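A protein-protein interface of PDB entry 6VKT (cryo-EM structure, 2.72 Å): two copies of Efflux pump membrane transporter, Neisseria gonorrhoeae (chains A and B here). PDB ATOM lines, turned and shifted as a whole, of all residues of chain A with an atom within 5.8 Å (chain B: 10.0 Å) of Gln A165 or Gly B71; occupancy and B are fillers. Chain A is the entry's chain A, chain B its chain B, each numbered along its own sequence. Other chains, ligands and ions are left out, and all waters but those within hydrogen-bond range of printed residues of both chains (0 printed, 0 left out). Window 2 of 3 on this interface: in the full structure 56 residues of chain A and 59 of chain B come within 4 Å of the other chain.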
ATOM      1  N   VAL A 160      13.519   7.197  21.998  1.00  0.00           N
ATOM      2  CA  VAL A 160      13.842   7.307  20.581  1.00  0.00           C
ATOM      3  C   VAL A 160      14.848   6.244  20.152  1.00  0.00           C
ATOM      4  O   VAL A 160      14.690   5.616  19.104  1.00  0.00           O
ATOM      5  CB  VAL A 160      14.355   8.724  20.238  1.00  0.00           C
ATOM      6  CG1 VAL A 160      14.681   8.824  18.759  1.00  0.00           C
ATOM      7  CG2 VAL A 160      13.325   9.769  20.632  1.00  0.00           C
ATOM      8  N   VAL A 161      15.893   6.031  20.953  1.00  0.00           N
ATOM      9  CA  VAL A 161      16.919   5.054  20.588  1.00  0.00           C
ATOM     10  C   VAL A 161      16.367   3.634  20.545  1.00  0.00           C
ATOM     11  O   VAL A 161      16.620   2.927  19.555  1.00  0.00           O
ATOM     12  CB  VAL A 161      18.130   5.185  21.527  1.00  0.00           C
ATOM     13  CG1 VAL A 161      19.140   4.086  21.244  1.00  0.00           C
ATOM     14  CG2 VAL A 161      18.772   6.553  21.373  1.00  0.00           C
ATOM     15  N   PRO A 162      15.648   3.144  21.560  1.00  0.00           N
ATOM     16  CA  PRO A 162      15.091   1.785  21.459  1.00  0.00           C
ATOM     17  C   PRO A 162      14.078   1.633  20.339  1.00  0.00           C
ATOM     18  O   PRO A 162      14.015   0.563  19.721  1.00  0.00           O
ATOM     19  CB  PRO A 162      14.446   1.565  22.835  1.00  0.00           C
ATOM     20  CG  PRO A 162      15.146   2.515  23.739  1.00  0.00           C
ATOM     21  CD  PRO A 162      15.451   3.717  22.903  1.00  0.00           C
ATOM     22  N   GLU A 163      13.283   2.667  20.058  1.00  0.00           N
ATOM     23  CA  GLU A 163      12.320   2.587  18.967  1.00  0.00           C
ATOM     24  C   GLU A 163      12.994   2.552  17.604  1.00  0.00           C
ATOM     25  O   GLU A 163      12.427   1.990  16.661  1.00  0.00           O
ATOM     26  CB  GLU A 163      11.350   3.766  19.037  1.00  0.00           C
ATOM     27  CG  GLU A 163      10.345   3.680  20.171  1.00  0.00           C
ATOM     28  CD  GLU A 163       9.134   2.842  19.812  1.00  0.00           C
ATOM     29  OE1 GLU A 163       8.882   2.648  18.605  1.00  0.00           O
ATOM     30  OE2 GLU A 163       8.434   2.379  20.736  1.00  0.00           O
ATOM     31  N   LEU A 164      14.186   3.131  17.479  1.00  0.00           N
ATOM     32  CA  LEU A 164      14.902   3.171  16.211  1.00  0.00           C
ATOM     33  C   LEU A 164      15.826   1.984  16.001  1.00  0.00           C
ATOM     34  O   LEU A 164      16.024   1.566  14.855  1.00  0.00           O
ATOM     35  CB  LEU A 164      15.721   4.463  16.104  1.00  0.00           C
ATOM     36  CG  LEU A 164      15.146   5.571  15.222  1.00  0.00           C
ATOM     37  CD1 LEU A 164      13.715   5.890  15.618  1.00  0.00           C
ATOM     38  CD2 LEU A 164      16.015   6.813  15.303  1.00  0.00           C
ATOM     39  N   GLN A 165      16.398   1.427  17.067  1.00  0.00           N
ATOM     40  CA  GLN A 165      17.324   0.311  16.915  1.00  0.00           C
ATOM     41  C   GLN A 165      16.622  -1.026  16.729  1.00  0.00           C
ATOM     42  O   GLN A 165      17.302  -2.044  16.570  1.00  0.00           O
ATOM     43  CB  GLN A 165      18.269   0.237  18.117  1.00  0.00           C
ATOM     44  CG  GLN A 165      17.585   0.021  19.450  1.00  0.00           C
ATOM     45  CD  GLN A 165      18.555   0.099  20.611  1.00  0.00           C
ATOM     46  OE1 GLN A 165      19.761   0.250  20.415  1.00  0.00           O
ATOM     47  NE2 GLN A 165      18.034  -0.005  21.828  1.00  0.00           N
ATOM     48  N   ARG A 166      15.288  -1.040  16.730  1.00  0.00           N
ATOM     49  CA  ARG A 166      14.532  -2.255  16.460  1.00  0.00           C
ATOM     50  C   ARG A 166      13.921  -2.260  15.064  1.00  0.00           C
ATOM     51  O   ARG A 166      13.102  -3.132  14.758  1.00  0.00           O
ATOM     52  CB  ARG A 166      13.443  -2.447  17.517  1.00  0.00           C
ATOM     53  CG  ARG A 166      12.223  -1.567  17.338  1.00  0.00           C
ATOM     54  CD  ARG A 166      11.052  -2.090  18.155  1.00  0.00           C
ATOM     55  NE  ARG A 166      11.320  -2.039  19.590  1.00  0.00           N
ATOM     56  CZ  ARG A 166      10.774  -1.157  20.420  1.00  0.00           C
ATOM     57  NH1 ARG A 166       9.918  -0.253  19.964  1.00  0.00           N
ATOM     58  NH2 ARG A 166      11.088  -1.174  21.710  1.00  0.00           N
ATOM     59  N   ILE A 167      14.299  -1.320  14.229  1.00  0.00           N
ATOM     60  CA  ILE A 167      13.851  -1.297  12.842  1.00  0.00           C
ATOM     61  C   ILE A 167      14.691  -2.274  12.031  1.00  0.00           C
ATOM     62  O   ILE A 167      15.904  -2.401  12.245  1.00  0.00           O
ATOM     63  CB  ILE A 167      13.942   0.127  12.268  1.00  0.00           C
ATOM     64  CG1 ILE A 167      13.013   1.074  13.030  1.00  0.00           C
ATOM     65  CG2 ILE A 167      13.613   0.130  10.786  1.00  0.00           C
ATOM     66  CD1 ILE A 167      11.552   0.709  12.921  1.00  0.00           C
ATOM     67  N   VAL A 170      18.597  -1.679  10.691  1.00  0.00           N
ATOM     68  CA  VAL A 170      19.438  -0.869  11.564  1.00  0.00           C
ATOM     69  C   VAL A 170      20.420  -1.778  12.289  1.00  0.00           C
ATOM     70  O   VAL A 170      20.039  -2.828  12.821  1.00  0.00           O
ATOM     71  CB  VAL A 170      18.581  -0.071  12.559  1.00  0.00           C
ATOM     72  CG1 VAL A 170      19.467   0.725  13.500  1.00  0.00           C
ATOM     73  CG2 VAL A 170      17.624   0.846  11.816  1.00  0.00           C
ATOM     74  N   GLN A 172      23.119  -0.277  14.398  1.00  0.00           N
ATOM     75  CA  GLN A 172      23.561   0.383  15.617  1.00  0.00           C
ATOM     76  C   GLN A 172      23.071   1.821  15.605  1.00  0.00           C
ATOM     77  O   GLN A 172      22.958   2.435  14.541  1.00  0.00           O
ATOM     78  CB  GLN A 172      25.087   0.339  15.752  1.00  0.00           C
ATOM     79  CG  GLN A 172      25.608   0.872  17.073  1.00  0.00           C
ATOM     80  CD  GLN A 172      27.093   0.635  17.250  1.00  0.00           C
ATOM     81  OE1 GLN A 172      27.870   1.578  17.401  1.00  0.00           O
ATOM     82  NE2 GLN A 172      27.496  -0.629  17.229  1.00  0.00           N
ATOM     83  N   VAL A 173      22.782   2.350  16.790  1.00  0.00           N
ATOM     84  CA  VAL A 173      22.332   3.728  16.960  1.00  0.00           C
ATOM     85  C   VAL A 173      23.216   4.345  18.037  1.00  0.00           C
ATOM     86  O   VAL A 173      23.033   4.077  19.229  1.00  0.00           O
ATOM     87  CB  VAL A 173      20.851   3.821  17.341  1.00  0.00           C
ATOM     88  CG1 VAL A 173      20.438   5.273  17.505  1.00  0.00           C
ATOM     89  CG2 VAL A 173      19.991   3.134  16.292  1.00  0.00           C
ATOM     90  N   ILE B  65      16.621  -6.398  31.573  1.00  0.00           N
ATOM     91  CA  ILE B  65      16.784  -7.367  30.496  1.00  0.00           C
ATOM     92  C   ILE B  65      16.085  -6.901  29.223  1.00  0.00           C
ATOM     93  O   ILE B  65      16.538  -7.209  28.114  1.00  0.00           O
ATOM     94  CB  ILE B  65      16.272  -8.748  30.934  1.00  0.00           C
ATOM     95  CG1 ILE B  65      17.018  -9.224  32.181  1.00  0.00           C
ATOM     96  CG2 ILE B  65      16.437  -9.749  29.808  1.00  0.00           C
ATOM     97  CD1 ILE B  65      16.550 -10.565  32.697  1.00  0.00           C
ATOM     98  N   GLU B  66      14.984  -6.158  29.351  1.00  0.00           N
ATOM     99  CA  GLU B  66      14.239  -5.721  28.178  1.00  0.00           C
ATOM    100  C   GLU B  66      14.955  -4.587  27.454  1.00  0.00           C
ATOM    101  O   GLU B  66      14.909  -4.505  26.221  1.00  0.00           O
ATOM    102  CB  GLU B  66      12.831  -5.292  28.588  1.00  0.00           C
ATOM    103  CG  GLU B  66      11.904  -4.987  27.427  1.00  0.00           C
ATOM    104  CD  GLU B  66      10.594  -4.370  27.879  1.00  0.00           C
ATOM    105  OE1 GLU B  66      10.600  -3.648  28.899  1.00  0.00           O
ATOM    106  OE2 GLU B  66       9.562  -4.607  27.218  1.00  0.00           O
ATOM    107  N   ARG B  67      15.623  -3.705  28.198  1.00  0.00           N
ATOM    108  CA  ARG B  67      16.323  -2.594  27.565  1.00  0.00           C
ATOM    109  C   ARG B  67      17.588  -3.027  26.834  1.00  0.00           C
ATOM    110  O   ARG B  67      18.208  -2.193  26.166  1.00  0.00           O
ATOM    111  CB  ARG B  67      16.659  -1.522  28.602  1.00  0.00           C
ATOM    112  CG  ARG B  67      17.662  -1.953  29.656  1.00  0.00           C
ATOM    113  CD  ARG B  67      18.091  -0.769  30.508  1.00  0.00           C
ATOM    114  NE  ARG B  67      16.945  -0.077  31.089  1.00  0.00           N
ATOM    115  CZ  ARG B  67      16.567  -0.191  32.358  1.00  0.00           C
ATOM    116  NH1 ARG B  67      17.478  -0.308  33.315  1.00  0.00           N
ATOM    117  NH2 ARG B  67      15.280  -0.191  32.672  1.00  0.00           N
ATOM    118  N   ASN B  68      17.986  -4.296  26.942  1.00  0.00           N
ATOM    119  CA  ASN B  68      19.112  -4.824  26.187  1.00  0.00           C
ATOM    120  C   ASN B  68      18.697  -5.717  25.027  1.00  0.00           C
ATOM    121  O   ASN B  68      19.535  -6.011  24.169  1.00  0.00           O
ATOM    122  CB  ASN B  68      20.051  -5.616  27.109  1.00  0.00           C
ATOM    123  CG  ASN B  68      21.425  -5.822  26.503  1.00  0.00           C
ATOM    124  OD1 ASN B  68      21.922  -4.976  25.760  1.00  0.00           O
ATOM    125  ND2 ASN B  68      22.047  -6.952  26.815  1.00  0.00           N
ATOM    126  N   MET B  69      17.441  -6.148  24.977  1.00  0.00           N
ATOM    127  CA  MET B  69      16.945  -6.982  23.883  1.00  0.00           C
ATOM    128  C   MET B  69      16.389  -6.133  22.745  1.00  0.00           C
ATOM    129  O   MET B  69      15.268  -6.331  22.278  1.00  0.00           O
ATOM    130  CB  MET B  69      15.892  -7.952  24.405  1.00  0.00           C
ATOM    131  CG  MET B  69      16.399  -8.903  25.474  1.00  0.00           C
ATOM    132  SD  MET B  69      17.671 -10.021  24.862  1.00  0.00           S
ATOM    133  CE  MET B  69      18.070 -10.922  26.355  1.00  0.00           C
ATOM    134  N   ASN B  70      17.186  -5.172  22.287  1.00  0.00           N
ATOM    135  CA  ASN B  70      16.822  -4.302  21.176  1.00  0.00           C
ATOM    136  C   ASN B  70      17.913  -4.398  20.124  1.00  0.00           C
ATOM    137  O   ASN B  70      19.077  -4.092  20.404  1.00  0.00           O
ATOM    138  CB  ASN B  70      16.639  -2.853  21.638  1.00  0.00           C
ATOM    139  CG  ASN B  70      15.338  -2.640  22.385  1.00  0.00           C
ATOM    140  OD1 ASN B  70      14.300  -3.185  22.014  1.00  0.00           O
ATOM    141  ND2 ASN B  70      15.390  -1.844  23.446  1.00  0.00           N
ATOM    142  N   GLY B  71      17.541  -4.822  18.922  1.00  0.00           N
ATOM    143  CA  GLY B  71      18.489  -5.045  17.846  1.00  0.00           C
ATOM    144  C   GLY B  71      18.576  -6.478  17.377  1.00  0.00           C
ATOM    145  O   GLY B  71      19.301  -6.753  16.409  1.00  0.00           O
ATOM    146  N   VAL B  72      17.874  -7.410  18.021  1.00  0.00           N
ATOM    147  CA  VAL B  72      17.869  -8.794  17.568  1.00  0.00           C
ATOM    148  C   VAL B  72      17.182  -8.871  16.212  1.00  0.00           C
ATOM    149  O   VAL B  72      16.084  -8.332  16.024  1.00  0.00           O
ATOM    150  CB  VAL B  72      17.179  -9.697  18.600  1.00  0.00           C
ATOM    151  CG1 VAL B  72      17.268 -11.153  18.173  1.00  0.00           C
ATOM    152  CG2 VAL B  72      17.799  -9.499  19.973  1.00  0.00           C
ATOM    153  N   GLU B  73      17.829  -9.539  15.261  1.00  0.00           N
ATOM    154  CA  GLU B  73      17.312  -9.613  13.901  1.00  0.00           C
ATOM    155  C   GLU B  73      15.998 -10.385  13.877  1.00  0.00           C
ATOM    156  O   GLU B  73      15.953 -11.562  14.252  1.00  0.00           O
ATOM    157  CB  GLU B  73      18.338 -10.273  12.984  1.00  0.00           C
ATOM    158  CG  GLU B  73      18.152  -9.952  11.511  1.00  0.00           C
ATOM    159  CD  GLU B  73      18.717 -11.029  10.605  1.00  0.00           C
ATOM    160  OE1 GLU B  73      19.085 -12.105  11.118  1.00  0.00           O
ATOM    161  OE2 GLU B  73      18.792 -10.797   9.380  1.00  0.00           O
ATOM    162  N   GLY B  74      14.933  -9.724  13.440  1.00  0.00           N
ATOM    163  CA  GLY B  74      13.636 -10.351  13.323  1.00  0.00           C
ATOM    164  C   GLY B  74      12.716 -10.192  14.512  1.00  0.00           C
ATOM    165  O   GLY B  74      11.742 -10.946  14.616  1.00  0.00           O
ATOM    166  N   LEU B  75      12.987  -9.245  15.405  1.00  0.00           N
ATOM    167  CA  LEU B  75      12.148  -9.043  16.580  1.00  0.00           C
ATOM    168  C   LEU B  75      10.872  -8.315  16.180  1.00  0.00           C
ATOM    169  O   LEU B  75      10.926  -7.207  15.635  1.00  0.00           O
ATOM    170  CB  LEU B  75      12.904  -8.256  17.648  1.00  0.00           C
ATOM    171  CG  LEU B  75      12.099  -7.889  18.896  1.00  0.00           C
ATOM    172  CD1 LEU B  75      11.637  -9.140  19.625  1.00  0.00           C
ATOM    173  CD2 LEU B  75      12.908  -6.995  19.820  1.00  0.00           C
ATOM    174  N   ASP B  76       9.725  -8.938  16.449  1.00  0.00           N
ATOM    175  CA  ASP B  76       8.432  -8.318  16.177  1.00  0.00           C
ATOM    176  C   ASP B  76       8.010  -7.407  17.327  1.00  0.00           C
ATOM    177  O   ASP B  76       7.774  -6.210  17.127  1.00  0.00           O
ATOM    178  CB  ASP B  76       7.375  -9.398  15.923  1.00  0.00           C
ATOM    179  CG  ASP B  76       6.104  -8.838  15.320  1.00  0.00           C
ATOM    180  OD1 ASP B  76       6.085  -7.637  14.978  1.00  0.00           O
ATOM    181  OD2 ASP B  76       5.122  -9.598  15.188  1.00  0.00           O
ATOM    182  N   MET B  78       7.849  -7.323  22.112  1.00  0.00           N
ATOM    183  CA  MET B  78       8.267  -7.931  23.365  1.00  0.00           C
ATOM    184  C   MET B  78       7.333  -7.487  24.478  1.00  0.00           C
ATOM    185  O   MET B  78       6.799  -6.375  24.456  1.00  0.00           O
ATOM    186  CB  MET B  78       9.716  -7.568  23.711  1.00  0.00           C
ATOM    187  CG  MET B  78       9.979  -6.075  23.765  1.00  0.00           C
ATOM    188  SD  MET B  78      11.710  -5.681  24.074  1.00  0.00           S
ATOM    189  CE  MET B  78      11.659  -3.893  24.018  1.00  0.00           C
ATOM    190  N   LEU B  92       9.668 -12.483  24.052  1.00  0.00           N
ATOM    191  CA  LEU B  92      10.032 -11.820  22.807  1.00  0.00           C
ATOM    192  C   LEU B  92       9.385 -12.588  21.662  1.00  0.00           C
ATOM    193  O   LEU B  92       9.721 -13.753  21.425  1.00  0.00           O
ATOM    194  CB  LEU B  92      11.547 -11.764  22.633  1.00  0.00           C
ATOM    195  CG  LEU B  92      12.360 -10.839  23.538  1.00  0.00           C
ATOM    196  CD1 LEU B  92      12.505 -11.428  24.931  1.00  0.00           C
ATOM    197  CD2 LEU B  92      13.723 -10.577  22.924  1.00  0.00           C
ATOM    198  N   PHE B  94       9.018 -12.925  17.723  1.00  0.00           N
ATOM    199  CA  PHE B  94       9.880 -12.602  16.598  1.00  0.00           C
ATOM    200  C   PHE B  94       9.082 -12.529  15.302  1.00  0.00           C
ATOM    201  O   PHE B  94       8.072 -13.215  15.128  1.00  0.00           O
ATOM    202  CB  PHE B  94      10.999 -13.636  16.460  1.00  0.00           C
ATOM    203  CG  PHE B  94      12.079 -13.498  17.494  1.00  0.00           C
ATOM    204  CD1 PHE B  94      11.939 -14.076  18.742  1.00  0.00           C
ATOM    205  CD2 PHE B  94      13.234 -12.786  17.218  1.00  0.00           C
ATOM    206  CE1 PHE B  94      12.927 -13.949  19.696  1.00  0.00           C
ATOM    207  CE2 PHE B  94      14.226 -12.656  18.168  1.00  0.00           C
ATOM    208  CZ  PHE B  94      14.073 -13.239  19.408  1.00  0.00           C
ATOM    209  N   LEU B 102      18.296 -19.657  15.936  1.00  0.00           N
ATOM    210  CA  LEU B 102      19.107 -18.447  15.869  1.00  0.00           C
ATOM    211  C   LEU B 102      18.563 -17.373  16.801  1.00  0.00           C
ATOM    212  O   LEU B 102      19.333 -16.662  17.455  1.00  0.00           O
ATOM    213  CB  LEU B 102      19.166 -17.931  14.431  1.00  0.00           C
ATOM    214  CG  LEU B 102      20.271 -18.513  13.548  1.00  0.00           C
ATOM    215  CD1 LEU B 102      21.639 -18.231  14.150  1.00  0.00           C
ATOM    216  CD2 LEU B 102      20.068 -20.004  13.341  1.00  0.00           C
ATOM    217  N   ALA B 103      17.238 -17.246  16.882  1.00  0.00           N
ATOM    218  CA  ALA B 103      16.645 -16.280  17.799  1.00  0.00           C
ATOM    219  C   ALA B 103      16.997 -16.608  19.244  1.00  0.00           C
ATOM    220  O   ALA B 103      17.338 -15.711  20.025  1.00  0.00           O
ATOM    221  CB  ALA B 103      15.130 -16.239  17.609  1.00  0.00           C
ATOM    222  N   GLU B 106      20.691 -15.854  19.889  1.00  0.00           N
ATOM    223  CA  GLU B 106      20.869 -14.408  19.975  1.00  0.00           C
ATOM    224  C   GLU B 106      20.376 -13.868  21.310  1.00  0.00           C
ATOM    225  O   GLU B 106      21.021 -13.003  21.915  1.00  0.00           O
ATOM    226  CB  GLU B 106      20.146 -13.717  18.820  1.00  0.00           C
ATOM    227  CG  GLU B 106      20.711 -14.029  17.447  1.00  0.00           C
ATOM    228  CD  GLU B 106      20.178 -13.098  16.376  1.00  0.00           C
ATOM    229  OE1 GLU B 106      20.657 -11.947  16.296  1.00  0.00           O
ATOM    230  OE2 GLU B 106      19.280 -13.516  15.616  1.00  0.00           O
ATOM    231  N   VAL B 107      19.228 -14.360  21.784  1.00  0.00           N
ATOM    232  CA  VAL B 107      18.705 -13.907  23.071  1.00  0.00           C
ATOM    233  C   VAL B 107      19.645 -14.309  24.199  1.00  0.00           C
ATOM    234  O   VAL B 107      19.888 -13.534  25.131  1.00  0.00           O
ATOM    235  CB  VAL B 107      17.284 -14.453  23.293  1.00  0.00           C
ATOM    236  CG1 VAL B 107      16.803 -14.122  24.697  1.00  0.00           C
ATOM    237  CG2 VAL B 107      16.333 -13.889  22.253  1.00  0.00           C
ATOM    238  N   LYS B 110      22.637 -11.989  24.107  1.00  0.00           N
ATOM    239  CA  LYS B 110      22.296 -10.667  24.620  1.00  0.00           C
ATOM    240  C   LYS B 110      22.108 -10.684  26.131  1.00  0.00           C
ATOM    241  O   LYS B 110      22.400  -9.688  26.801  1.00  0.00           O
ATOM    242  CB  LYS B 110      21.034 -10.144  23.935  1.00  0.00           C
ATOM    243  CG  LYS B 110      21.246  -9.682  22.505  1.00  0.00           C
ATOM    244  CD  LYS B 110      22.224  -8.521  22.438  1.00  0.00           C
ATOM    245  CE  LYS B 110      22.372  -8.005  21.017  1.00  0.00           C
ATOM    246  NZ  LYS B 110      21.088  -7.474  20.484  1.00  0.00           N
ATOM    247  N   GLU B 113      25.589 -10.701  28.361  1.00  0.00           N
ATOM    248  CA  GLU B 113      26.326  -9.459  28.554  1.00  0.00           C
ATOM    249  C   GLU B 113      25.676  -8.520  29.560  1.00  0.00           C
ATOM    250  O   GLU B 113      26.230  -7.450  29.832  1.00  0.00           O
ATOM    251  CB  GLU B 113      26.495  -8.730  27.217  1.00  0.00           C
ATOM    252  CG  GLU B 113      25.193  -8.294  26.572  1.00  0.00           C
ATOM    253  CD  GLU B 113      25.389  -7.776  25.162  1.00  0.00           C
ATOM    254  OE1 GLU B 113      26.409  -8.130  24.534  1.00  0.00           O
ATOM    255  OE2 GLU B 113      24.528  -7.012  24.682  1.00  0.00           O
ATOM    256  N   ASN B 817       6.711  -3.401  24.894  1.00  0.00           N
ATOM    257  CA  ASN B 817       7.658  -2.663  24.059  1.00  0.00           C
ATOM    258  C   ASN B 817       8.425  -1.613  24.856  1.00  0.00           C
ATOM    259  O   ASN B 817       8.807  -0.569  24.321  1.00  0.00           O
ATOM    260  CB  ASN B 817       6.955  -2.017  22.863  1.00  0.00           C
ATOM    261  CG  ASN B 817       6.657  -3.009  21.757  1.00  0.00           C
ATOM    262  OD1 ASN B 817       5.528  -3.107  21.281  1.00  0.00           O
ATOM    263  ND2 ASN B 817       7.674  -3.753  21.343  1.00  0.00           N
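The side-chain carboxylate (OE2) of Glu A163 is in salt-bridge range of the guanidinium group (NH1) of Arg A166, at 3.1 Å. The backbone carbonyl oxygen (O) of Met B78 is in hydrogen-bond range of the backbone NH (N) of Asn B817 (3.0 Å).
Among the printed residues, pairs that only touch across the chains: Gln A165 with Asn B70 (3.2 Å), Gln A165 with Gly B71 (3.5 Å), Arg A166 with Asn B817 (3.5 Å), Pro A162 with Asn B70 (3.6 Å), Arg A166 with Met B78 (3.6 Å) and Arg A166 with Asn B70 (3.8 Å).
Gly B71 touches just one residue of chain A: Gln A165 (3.5 Å). Pro A162 touches one residue of chain B. Leu A164 touches none of the printed residues of chain B. No residue of chain B comes within 4 Å of Val A173. Printed residues of chain A within 4 Å of Asn B817: Arg A166 (3.5 Å). Printed residues of chain A within 4 Å of Asn B70: Pro A162, Gln A165 and Arg A166. Val B72 touches none of the printed residues of chain A. The nearest residue of chain B that does not touch Gln A165 is Arg B67 (4.9 Å). The nearest residue of chain A that does not touch Gly B71 is Arg A166 (4.7 Å).
Printed residues of chain A that touch a printed residue of chain B: Pro A162, Gln A165 and Arg A166. Among the printed residues, no Asp or Glu carboxylate lies within 4 Å of a Lys or Arg side-chain nitrogen of the other chain.
No position is printed for both chains. Of the 6 pairs that touch across the chains among the printed residues, none has its exchanged pair printed and touching as well.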
